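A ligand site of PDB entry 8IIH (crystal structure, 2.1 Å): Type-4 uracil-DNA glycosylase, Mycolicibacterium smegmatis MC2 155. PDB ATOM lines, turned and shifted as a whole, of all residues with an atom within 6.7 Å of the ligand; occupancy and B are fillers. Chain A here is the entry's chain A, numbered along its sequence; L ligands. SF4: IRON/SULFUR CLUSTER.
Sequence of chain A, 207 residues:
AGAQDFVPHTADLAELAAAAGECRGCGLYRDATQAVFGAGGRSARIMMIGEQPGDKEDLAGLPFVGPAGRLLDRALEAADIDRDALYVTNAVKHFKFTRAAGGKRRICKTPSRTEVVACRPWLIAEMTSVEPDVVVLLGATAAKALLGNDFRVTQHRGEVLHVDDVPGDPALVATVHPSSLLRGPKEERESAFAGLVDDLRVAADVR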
ATOM      1  N   GLY A   2      -4.152  -0.003  -4.245  1.00  0.00           N
ATOM      2  CA  GLY A   2      -3.138   1.032  -4.528  1.00  0.00           C
ATOM      3  C   GLY A   2      -2.767   1.144  -6.008  1.00  0.00           C
ATOM      4  O   GLY A   2      -3.652   1.394  -6.810  1.00  0.00           O
ATOM      5  N   ALA A   3      -1.503   0.918  -6.337  1.00  0.00           N
ATOM      6  CA  ALA A   3      -1.011   1.043  -7.727  1.00  0.00           C
ATOM      7  C   ALA A   3      -1.135  -0.268  -8.497  1.00  0.00           C
ATOM      8  O   ALA A   3      -0.842  -0.230  -9.677  1.00  0.00           O
ATOM      9  CB  ALA A   3       0.416   1.498  -7.702  1.00  0.00           C
ATOM     10  N   PHE A   6      -2.433  -0.340 -12.105  1.00  0.00           N
ATOM     11  CA  PHE A   6      -1.623   0.545 -12.975  1.00  0.00           C
ATOM     12  C   PHE A   6      -0.324  -0.163 -13.434  1.00  0.00           C
ATOM     13  O   PHE A   6       0.249   0.292 -14.408  1.00  0.00           O
ATOM     14  CB  PHE A   6      -1.428   1.881 -12.265  1.00  0.00           C
ATOM     15  CG  PHE A   6      -2.679   2.664 -11.975  1.00  0.00           C
ATOM     16  CD1 PHE A   6      -3.329   3.349 -12.982  1.00  0.00           C
ATOM     17  CD2 PHE A   6      -3.182   2.750 -10.692  1.00  0.00           C
ATOM     18  CE1 PHE A   6      -4.475   4.079 -12.709  1.00  0.00           C
ATOM     19  CE2 PHE A   6      -4.332   3.467 -10.419  1.00  0.00           C
ATOM     20  CZ  PHE A   6      -4.979   4.136 -11.431  1.00  0.00           C
ATOM     21  N   ALA A  20       4.036   3.950 -15.022  1.00  0.00           N
ATOM     22  CA  ALA A  20       4.105   4.726 -13.770  1.00  0.00           C
ATOM     23  C   ALA A  20       3.705   6.179 -14.050  1.00  0.00           C
ATOM     24  O   ALA A  20       3.129   6.796 -13.155  1.00  0.00           O
ATOM     25  CB  ALA A  20       5.465   4.587 -13.145  1.00  0.00           C
ATOM     26  N   GLY A  21       3.992   6.676 -15.259  1.00  0.00           N
ATOM     27  CA  GLY A  21       3.518   8.010 -15.607  1.00  0.00           C
ATOM     28  C   GLY A  21       2.010   8.148 -15.565  1.00  0.00           C
ATOM     29  O   GLY A  21       1.508   9.255 -15.397  1.00  0.00           O
ATOM     30  N   GLU A  22       1.278   7.037 -15.701  1.00  0.00           N
ATOM     31  CA  GLU A  22      -0.184   7.077 -15.644  1.00  0.00           C
ATOM     32  C   GLU A  22      -0.757   6.672 -14.296  1.00  0.00           C
ATOM     33  O   GLU A  22      -1.986   6.669 -14.152  1.00  0.00           O
ATOM     34  CB  GLU A  22      -0.780   6.171 -16.733  1.00  0.00           C
ATOM     35  CG  GLU A  22      -0.044   6.242 -18.053  1.00  0.00           C
ATOM     36  CD  GLU A  22      -0.593   7.338 -18.944  1.00  0.00           C
ATOM     37  OE1 GLU A  22      -0.873   8.438 -18.426  1.00  0.00           O
ATOM     38  OE2 GLU A  22      -0.714   7.100 -20.169  1.00  0.00           O
ATOM     39  N   CYS A  23       0.068   6.329 -13.313  1.00  0.00           N
ATOM     40  CA  CYS A  23      -0.426   5.773 -12.065  1.00  0.00           C
ATOM     41  C   CYS A  23      -1.218   6.808 -11.277  1.00  0.00           C
ATOM     42  O   CYS A  23      -0.840   7.989 -11.221  1.00  0.00           O
ATOM     43  CB  CYS A  23       0.750   5.264 -11.211  1.00  0.00           C
ATOM     44  SG  CYS A  23       0.305   4.483  -9.644  1.00  0.00           S
ATOM     45  N   ARG A  24      -2.346   6.372 -10.681  1.00  0.00           N
ATOM     46  CA  ARG A  24      -3.100   7.181  -9.731  1.00  0.00           C
ATOM     47  C   ARG A  24      -3.253   6.431  -8.408  1.00  0.00           C
ATOM     48  O   ARG A  24      -4.169   6.714  -7.625  1.00  0.00           O
ATOM     49  CB  ARG A  24      -4.456   7.590 -10.315  1.00  0.00           C
ATOM     50  CG  ARG A  24      -4.310   8.281 -11.692  1.00  0.00           C
ATOM     51  CD  ARG A  24      -5.615   8.860 -12.236  1.00  0.00           C
ATOM     52  NE  ARG A  24      -6.730   7.940 -12.067  1.00  0.00           N
ATOM     53  CZ  ARG A  24      -7.074   6.997 -12.942  1.00  0.00           C
ATOM     54  NH1 ARG A  24      -6.389   6.800 -14.057  1.00  0.00           N
ATOM     55  NH2 ARG A  24      -8.139   6.242 -12.692  1.00  0.00           N
ATOM     56  N   GLY A  25      -2.340   5.508  -8.137  1.00  0.00           N
ATOM     57  CA  GLY A  25      -2.446   4.585  -7.014  1.00  0.00           C
ATOM     58  C   GLY A  25      -2.606   5.235  -5.658  1.00  0.00           C
ATOM     59  O   GLY A  25      -3.121   4.599  -4.737  1.00  0.00           O
ATOM     60  N   CYS A  26      -2.169   6.488  -5.508  1.00  0.00           N
ATOM     61  CA  CYS A  26      -2.420   7.300  -4.320  1.00  0.00           C
ATOM     62  C   CYS A  26      -2.587   8.739  -4.794  1.00  0.00           C
ATOM     63  O   CYS A  26      -2.612   9.008  -5.991  1.00  0.00           O
ATOM     64  CB  CYS A  26      -1.315   7.130  -3.267  1.00  0.00           C
ATOM     65  SG  CYS A  26       0.310   7.853  -3.707  1.00  0.00           S
ATOM     66  N   GLY A  27      -2.730   9.683  -3.872  1.00  0.00           N
ATOM     67  CA  GLY A  27      -2.919  11.049  -4.339  1.00  0.00           C
ATOM     68  C   GLY A  27      -1.678  11.794  -4.817  1.00  0.00           C
ATOM     69  O   GLY A  27      -1.803  12.934  -5.281  1.00  0.00           O
ATOM     70  N   LEU A  28      -0.488  11.195  -4.735  1.00  0.00           N
ATOM     71  CA  LEU A  28       0.739  11.984  -4.921  1.00  0.00           C
ATOM     72  C   LEU A  28       0.967  12.418  -6.369  1.00  0.00           C
ATOM     73  O   LEU A  28       1.717  13.377  -6.576  1.00  0.00           O
ATOM     74  CB  LEU A  28       1.948  11.197  -4.407  1.00  0.00           C
ATOM     75  CG  LEU A  28       1.884  11.045  -2.882  1.00  0.00           C
ATOM     76  CD1 LEU A  28       3.099  10.326  -2.320  1.00  0.00           C
ATOM     77  CD2 LEU A  28       1.694  12.418  -2.223  1.00  0.00           C
ATOM     78  N   TYR A  29       0.338  11.761  -7.343  1.00  0.00           N
ATOM     79  CA  TYR A  29       0.538  12.139  -8.743  1.00  0.00           C
ATOM     80  C   TYR A  29       0.029  13.540  -9.069  1.00  0.00           C
ATOM     81  O   TYR A  29       0.432  14.113 -10.093  1.00  0.00           O
ATOM     82  CB  TYR A  29      -0.159  11.132  -9.672  1.00  0.00           C
ATOM     83  CG  TYR A  29      -1.676  11.257  -9.659  1.00  0.00           C
ATOM     84  CD1 TYR A  29      -2.425  10.648  -8.655  1.00  0.00           C
ATOM     85  CD2 TYR A  29      -2.348  12.003 -10.637  1.00  0.00           C
ATOM     86  CE1 TYR A  29      -3.799  10.768  -8.624  1.00  0.00           C
ATOM     87  CE2 TYR A  29      -3.735  12.121 -10.607  1.00  0.00           C
ATOM     88  CZ  TYR A  29      -4.453  11.500  -9.606  1.00  0.00           C
ATOM     89  OH  TYR A  29      -5.819  11.611  -9.556  1.00  0.00           O
ATOM     90  N   ARG A  30      -0.919  14.059  -8.280  1.00  0.00           N
ATOM     91  CA  ARG A  30      -1.595  15.347  -8.589  1.00  0.00           C
ATOM     92  C   ARG A  30      -0.646  16.549  -8.598  1.00  0.00           C
ATOM     93  O   ARG A  30      -0.628  17.276  -9.582  1.00  0.00           O
ATOM     94  CB  ARG A  30      -2.767  15.577  -7.626  1.00  0.00           C
ATOM     95  CG  ARG A  30      -3.920  14.607  -7.794  1.00  0.00           C
ATOM     96  CD  ARG A  30      -5.120  15.095  -7.017  1.00  0.00           C
ATOM     97  NE  ARG A  30      -5.613  14.131  -6.040  1.00  0.00           N
ATOM     98  CZ  ARG A  30      -5.137  13.981  -4.802  1.00  0.00           C
ATOM     99  NH1 ARG A  30      -4.149  14.734  -4.367  1.00  0.00           N
ATOM    100  NH2 ARG A  30      -5.679  13.081  -4.006  1.00  0.00           N
ATOM    101  N   ALA A  35       6.134  11.183 -12.613  1.00  0.00           N
ATOM    102  CA  ALA A  35       6.598  10.015 -11.858  1.00  0.00           C
ATOM    103  C   ALA A  35       8.102   9.894 -12.098  1.00  0.00           C
ATOM    104  O   ALA A  35       8.543  10.220 -13.191  1.00  0.00           O
ATOM    105  CB  ALA A  35       5.912   8.779 -12.324  1.00  0.00           C
ATOM    106  N   ALA A  91      11.028   4.369  -2.809  1.00  0.00           N
ATOM    107  CA  ALA A  91       9.838   3.675  -2.277  1.00  0.00           C
ATOM    108  C   ALA A  91       8.562   4.241  -2.904  1.00  0.00           C
ATOM    109  O   ALA A  91       7.687   3.467  -3.241  1.00  0.00           O
ATOM    110  CB  ALA A  91       9.850   3.780  -0.785  1.00  0.00           C
ATOM    111  N   VAL A  92       8.442   5.558  -2.984  1.00  0.00           N
ATOM    112  CA  VAL A  92       7.316   6.104  -3.737  1.00  0.00           C
ATOM    113  C   VAL A  92       7.884   6.923  -4.885  1.00  0.00           C
ATOM    114  O   VAL A  92       9.031   7.397  -4.826  1.00  0.00           O
ATOM    115  CB  VAL A  92       6.334   6.932  -2.871  1.00  0.00           C
ATOM    116  CG1 VAL A  92       6.123   6.255  -1.529  1.00  0.00           C
ATOM    117  CG2 VAL A  92       6.768   8.389  -2.711  1.00  0.00           C
ATOM    118  N   LYS A  93       7.152   7.011  -6.001  1.00  0.00           N
ATOM    119  CA  LYS A  93       7.720   7.601  -7.251  1.00  0.00           C
ATOM    120  C   LYS A  93       7.187   9.003  -7.556  1.00  0.00           C
ATOM    121  O   LYS A  93       7.596   9.545  -8.572  1.00  0.00           O
ATOM    122  CB  LYS A  93       7.445   6.618  -8.390  1.00  0.00           C
ATOM    123  CG  LYS A  93       7.727   5.162  -8.079  1.00  0.00           C
ATOM    124  CD  LYS A  93       9.150   4.785  -8.316  1.00  0.00           C
ATOM    125  CE  LYS A  93       9.300   3.299  -8.508  1.00  0.00           C
ATOM    126  NZ  LYS A  93       9.695   2.646  -7.233  1.00  0.00           N
ATOM    127  N   HIS A  94       6.301   9.525  -6.726  1.00  0.00           N
ATOM    128  CA  HIS A  94       5.820  10.913  -6.899  1.00  0.00           C
ATOM    129  C   HIS A  94       6.286  11.785  -5.719  1.00  0.00           C
ATOM    130  O   HIS A  94       6.132  11.382  -4.592  1.00  0.00           O
ATOM    131  CB  HIS A  94       4.309  10.946  -7.141  1.00  0.00           C
ATOM    132  CG  HIS A  94       3.957  10.858  -8.574  1.00  0.00           C
ATOM    133  ND1 HIS A  94       3.367   9.757  -9.129  1.00  0.00           N
ATOM    134  CD2 HIS A  94       4.159  11.722  -9.564  1.00  0.00           C
ATOM    135  CE1 HIS A  94       3.174   9.956 -10.399  1.00  0.00           C
ATOM    136  NE2 HIS A  94       3.652  11.151 -10.672  1.00  0.00           N
ATOM    137  N   PHE A  95       6.818  12.945  -6.044  1.00  0.00           N
ATOM    138  CA  PHE A  95       7.323  13.865  -5.032  1.00  0.00           C
ATOM    139  C   PHE A  95       6.189  14.393  -4.171  1.00  0.00           C
ATOM    140  O   PHE A  95       5.229  14.972  -4.692  1.00  0.00           O
ATOM    141  CB  PHE A  95       8.019  15.028  -5.756  1.00  0.00           C
ATOM    142  CG  PHE A  95       8.698  16.018  -4.844  1.00  0.00           C
ATOM    143  CD1 PHE A  95       9.311  15.630  -3.679  1.00  0.00           C
ATOM    144  CD2 PHE A  95       8.721  17.365  -5.193  1.00  0.00           C
ATOM    145  CE1 PHE A  95       9.958  16.553  -2.859  1.00  0.00           C
ATOM    146  CE2 PHE A  95       9.366  18.304  -4.386  1.00  0.00           C
ATOM    147  CZ  PHE A  95       9.974  17.902  -3.220  1.00  0.00           C
ATOM    148  N   GLU A 115       0.673   5.590   1.641  1.00  0.00           N
ATOM    149  CA  GLU A 115       1.300   5.911   0.372  1.00  0.00           C
ATOM    150  C   GLU A 115       2.406   4.922   0.031  1.00  0.00           C
ATOM    151  O   GLU A 115       2.527   4.481  -1.115  1.00  0.00           O
ATOM    152  CB  GLU A 115       1.840   7.350   0.414  1.00  0.00           C
ATOM    153  CG  GLU A 115       0.740   8.401   0.201  1.00  0.00           C
ATOM    154  CD  GLU A 115       1.044   9.763   0.831  1.00  0.00           C
ATOM    155  OE1 GLU A 115       1.986   9.891   1.655  1.00  0.00           O
ATOM    156  OE2 GLU A 115       0.293  10.717   0.525  1.00  0.00           O
ATOM    157  N   ALA A 118       0.753   1.759  -0.981  1.00  0.00           N
ATOM    158  CA  ALA A 118       0.070   1.922  -2.266  1.00  0.00           C
ATOM    159  C   ALA A 118       1.047   1.762  -3.430  1.00  0.00           C
ATOM    160  O   ALA A 118       0.726   1.122  -4.432  1.00  0.00           O
ATOM    161  CB  ALA A 118      -0.626   3.268  -2.361  1.00  0.00           C
ATOM    162  N   CYS A 119       2.240   2.349  -3.305  1.00  0.00           N
ATOM    163  CA  CYS A 119       3.230   2.390  -4.369  1.00  0.00           C
ATOM    164  C   CYS A 119       4.113   1.144  -4.434  1.00  0.00           C
ATOM    165  O   CYS A 119       4.779   0.934  -5.452  1.00  0.00           O
ATOM    166  CB  CYS A 119       4.124   3.632  -4.211  1.00  0.00           C
ATOM    167  SG  CYS A 119       4.941   4.253  -5.715  1.00  0.00           S
ATOM    168  N   ARG A 120       4.134   0.331  -3.372  1.00  0.00           N
ATOM    169  CA  ARG A 120       5.016  -0.829  -3.349  1.00  0.00           C
ATOM    170  C   ARG A 120       4.867  -1.769  -4.551  1.00  0.00           C
ATOM    171  O   ARG A 120       5.884  -2.345  -4.948  1.00  0.00           O
ATOM    172  CB  ARG A 120       4.834  -1.614  -2.033  1.00  0.00           C
ATOM    173  CG  ARG A 120       5.943  -2.651  -1.773  1.00  0.00           C
ATOM    174  CD  ARG A 120       5.961  -3.233  -0.354  1.00  0.00           C
ATOM    175  NE  ARG A 120       4.618  -3.461   0.165  1.00  0.00           N
ATOM    176  CZ  ARG A 120       4.325  -3.644   1.453  1.00  0.00           C
ATOM    177  NH1 ARG A 120       5.260  -3.599   2.397  1.00  0.00           N
ATOM    178  NH2 ARG A 120       3.057  -3.859   1.803  1.00  0.00           N
ATOM    179  N   PRO A 121       3.687  -1.934  -5.177  1.00  0.00           N
ATOM    180  CA  PRO A 121       3.642  -2.718  -6.427  1.00  0.00           C
ATOM    181  C   PRO A 121       4.686  -2.326  -7.456  1.00  0.00           C
ATOM    182  O   PRO A 121       5.218  -3.206  -8.142  1.00  0.00           O
ATOM    183  CB  PRO A 121       2.221  -2.449  -6.949  1.00  0.00           C
ATOM    184  CG  PRO A 121       1.422  -2.223  -5.734  1.00  0.00           C
ATOM    185  CD  PRO A 121       2.318  -1.576  -4.720  1.00  0.00           C
ATOM    186  N   TRP A 122       5.007  -1.034  -7.603  1.00  0.00           N
ATOM    187  CA  TRP A 122       6.074  -0.647  -8.532  1.00  0.00           C
ATOM    188  C   TRP A 122       7.418  -1.176  -8.059  1.00  0.00           C
ATOM    189  O   TRP A 122       8.209  -1.708  -8.854  1.00  0.00           O
ATOM    190  CB  TRP A 122       6.150   0.875  -8.679  1.00  0.00           C
ATOM    191  CG  TRP A 122       4.967   1.460  -9.329  1.00  0.00           C
ATOM    192  CD1 TRP A 122       4.066   2.316  -8.771  1.00  0.00           C
ATOM    193  CD2 TRP A 122       4.532   1.247 -10.680  1.00  0.00           C
ATOM    194  NE1 TRP A 122       3.099   2.651  -9.678  1.00  0.00           N
ATOM    195  CE2 TRP A 122       3.355   2.003 -10.859  1.00  0.00           C
ATOM    196  CE3 TRP A 122       5.025   0.481 -11.742  1.00  0.00           C
ATOM    197  CZ2 TRP A 122       2.660   2.007 -12.065  1.00  0.00           C
ATOM    198  CZ3 TRP A 122       4.341   0.504 -12.942  1.00  0.00           C
ATOM    199  CH2 TRP A 122       3.168   1.267 -13.098  1.00  0.00           C
HETATM  200 FE1  SF4 L   1       3.331   5.641  -6.450  1.00  0.00          FE
HETATM  201 FE2  SF4 L   1       1.177   7.076  -5.642  1.00  0.00          FE
HETATM  202 FE3  SF4 L   1       1.158   5.825  -8.055  1.00  0.00          FE
HETATM  203 FE4  SF4 L   1       2.726   7.992  -7.661  1.00  0.00          FE
HETATM  204  S1  SF4 L   1       0.448   7.937  -7.636  1.00  0.00           S
HETATM  205  S2  SF4 L   1       3.344   6.057  -8.686  1.00  0.00           S
HETATM  206  S3  SF4 L   1       3.381   7.689  -5.488  1.00  0.00           S
HETATM  207  S4  SF4 L   1       1.221   4.843  -5.993  1.00  0.00           S
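CB of Ala 3 touches S4 of the ligand, 3.8 Å away.
Leu 28 touches the ligand (CB to S3, 3.9 Å).
Tyr 29 touches the ligand.
Lys 93 touches the ligand.
Hydrophobic or aromatic side chains that line the ligand: Ala 3, Leu 28, Tyr 29, His 94 and Trp 122.
The nearest printed residue that does not touch the ligand is Ala 118 (4.01 Å).
The side-chain sulfur of Cys 23 lies close to the backbone NH of Gly 25 (3.2 Å).
SG of Cys 23 lies close to NE1 of Trp 122 (3.3 Å).
The backbone NH (N) of Lys 93 lies close to the side-chain sulfur (SG) of Cys 119, at 3.5 Å.
The side-chain sulfur of Cys 119 sits close to the backbone carbonyl oxygen of Ala 91.
The backbone NH (N) of Leu 28 sits close to the side-chain sulfur (SG) of Cys 26 (3.6 Å).
A ring nitrogen (NE2) of His 94 is in hydrogen-bond range of the backbone NH (N) of Ala 35 (3.2 Å).
O of Ala 118 is in hydrogen-bond range of N of Ala 3 (2.9 Å).
The side-chain sulfur (SG) of Cys 23 is bound to an iron atom (FE3) of the ligand.
The side-chain sulfur (SG) of Cys 119 binds an iron atom (FE1) of the ligand, 2.2 Å away.
S1 of the ligand sits close to N of Cys 26 (3.7 Å).
FE2 of the ligand is bound by SG of Cys 26, 2.3 Å away.
S3 of the ligand sits close to N of His 94 (3.7 Å).
A ring nitrogen (ND1) of His 94 is bound to an iron atom (FE4) of the ligand (2.4 Å).
The backbone NH (N) of Gly 25 sits close to a sulfur (S1) of the ligand, at 3.7 Å.
NE1 of Trp 122 sits close to S2 of the ligand (3.6 Å).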
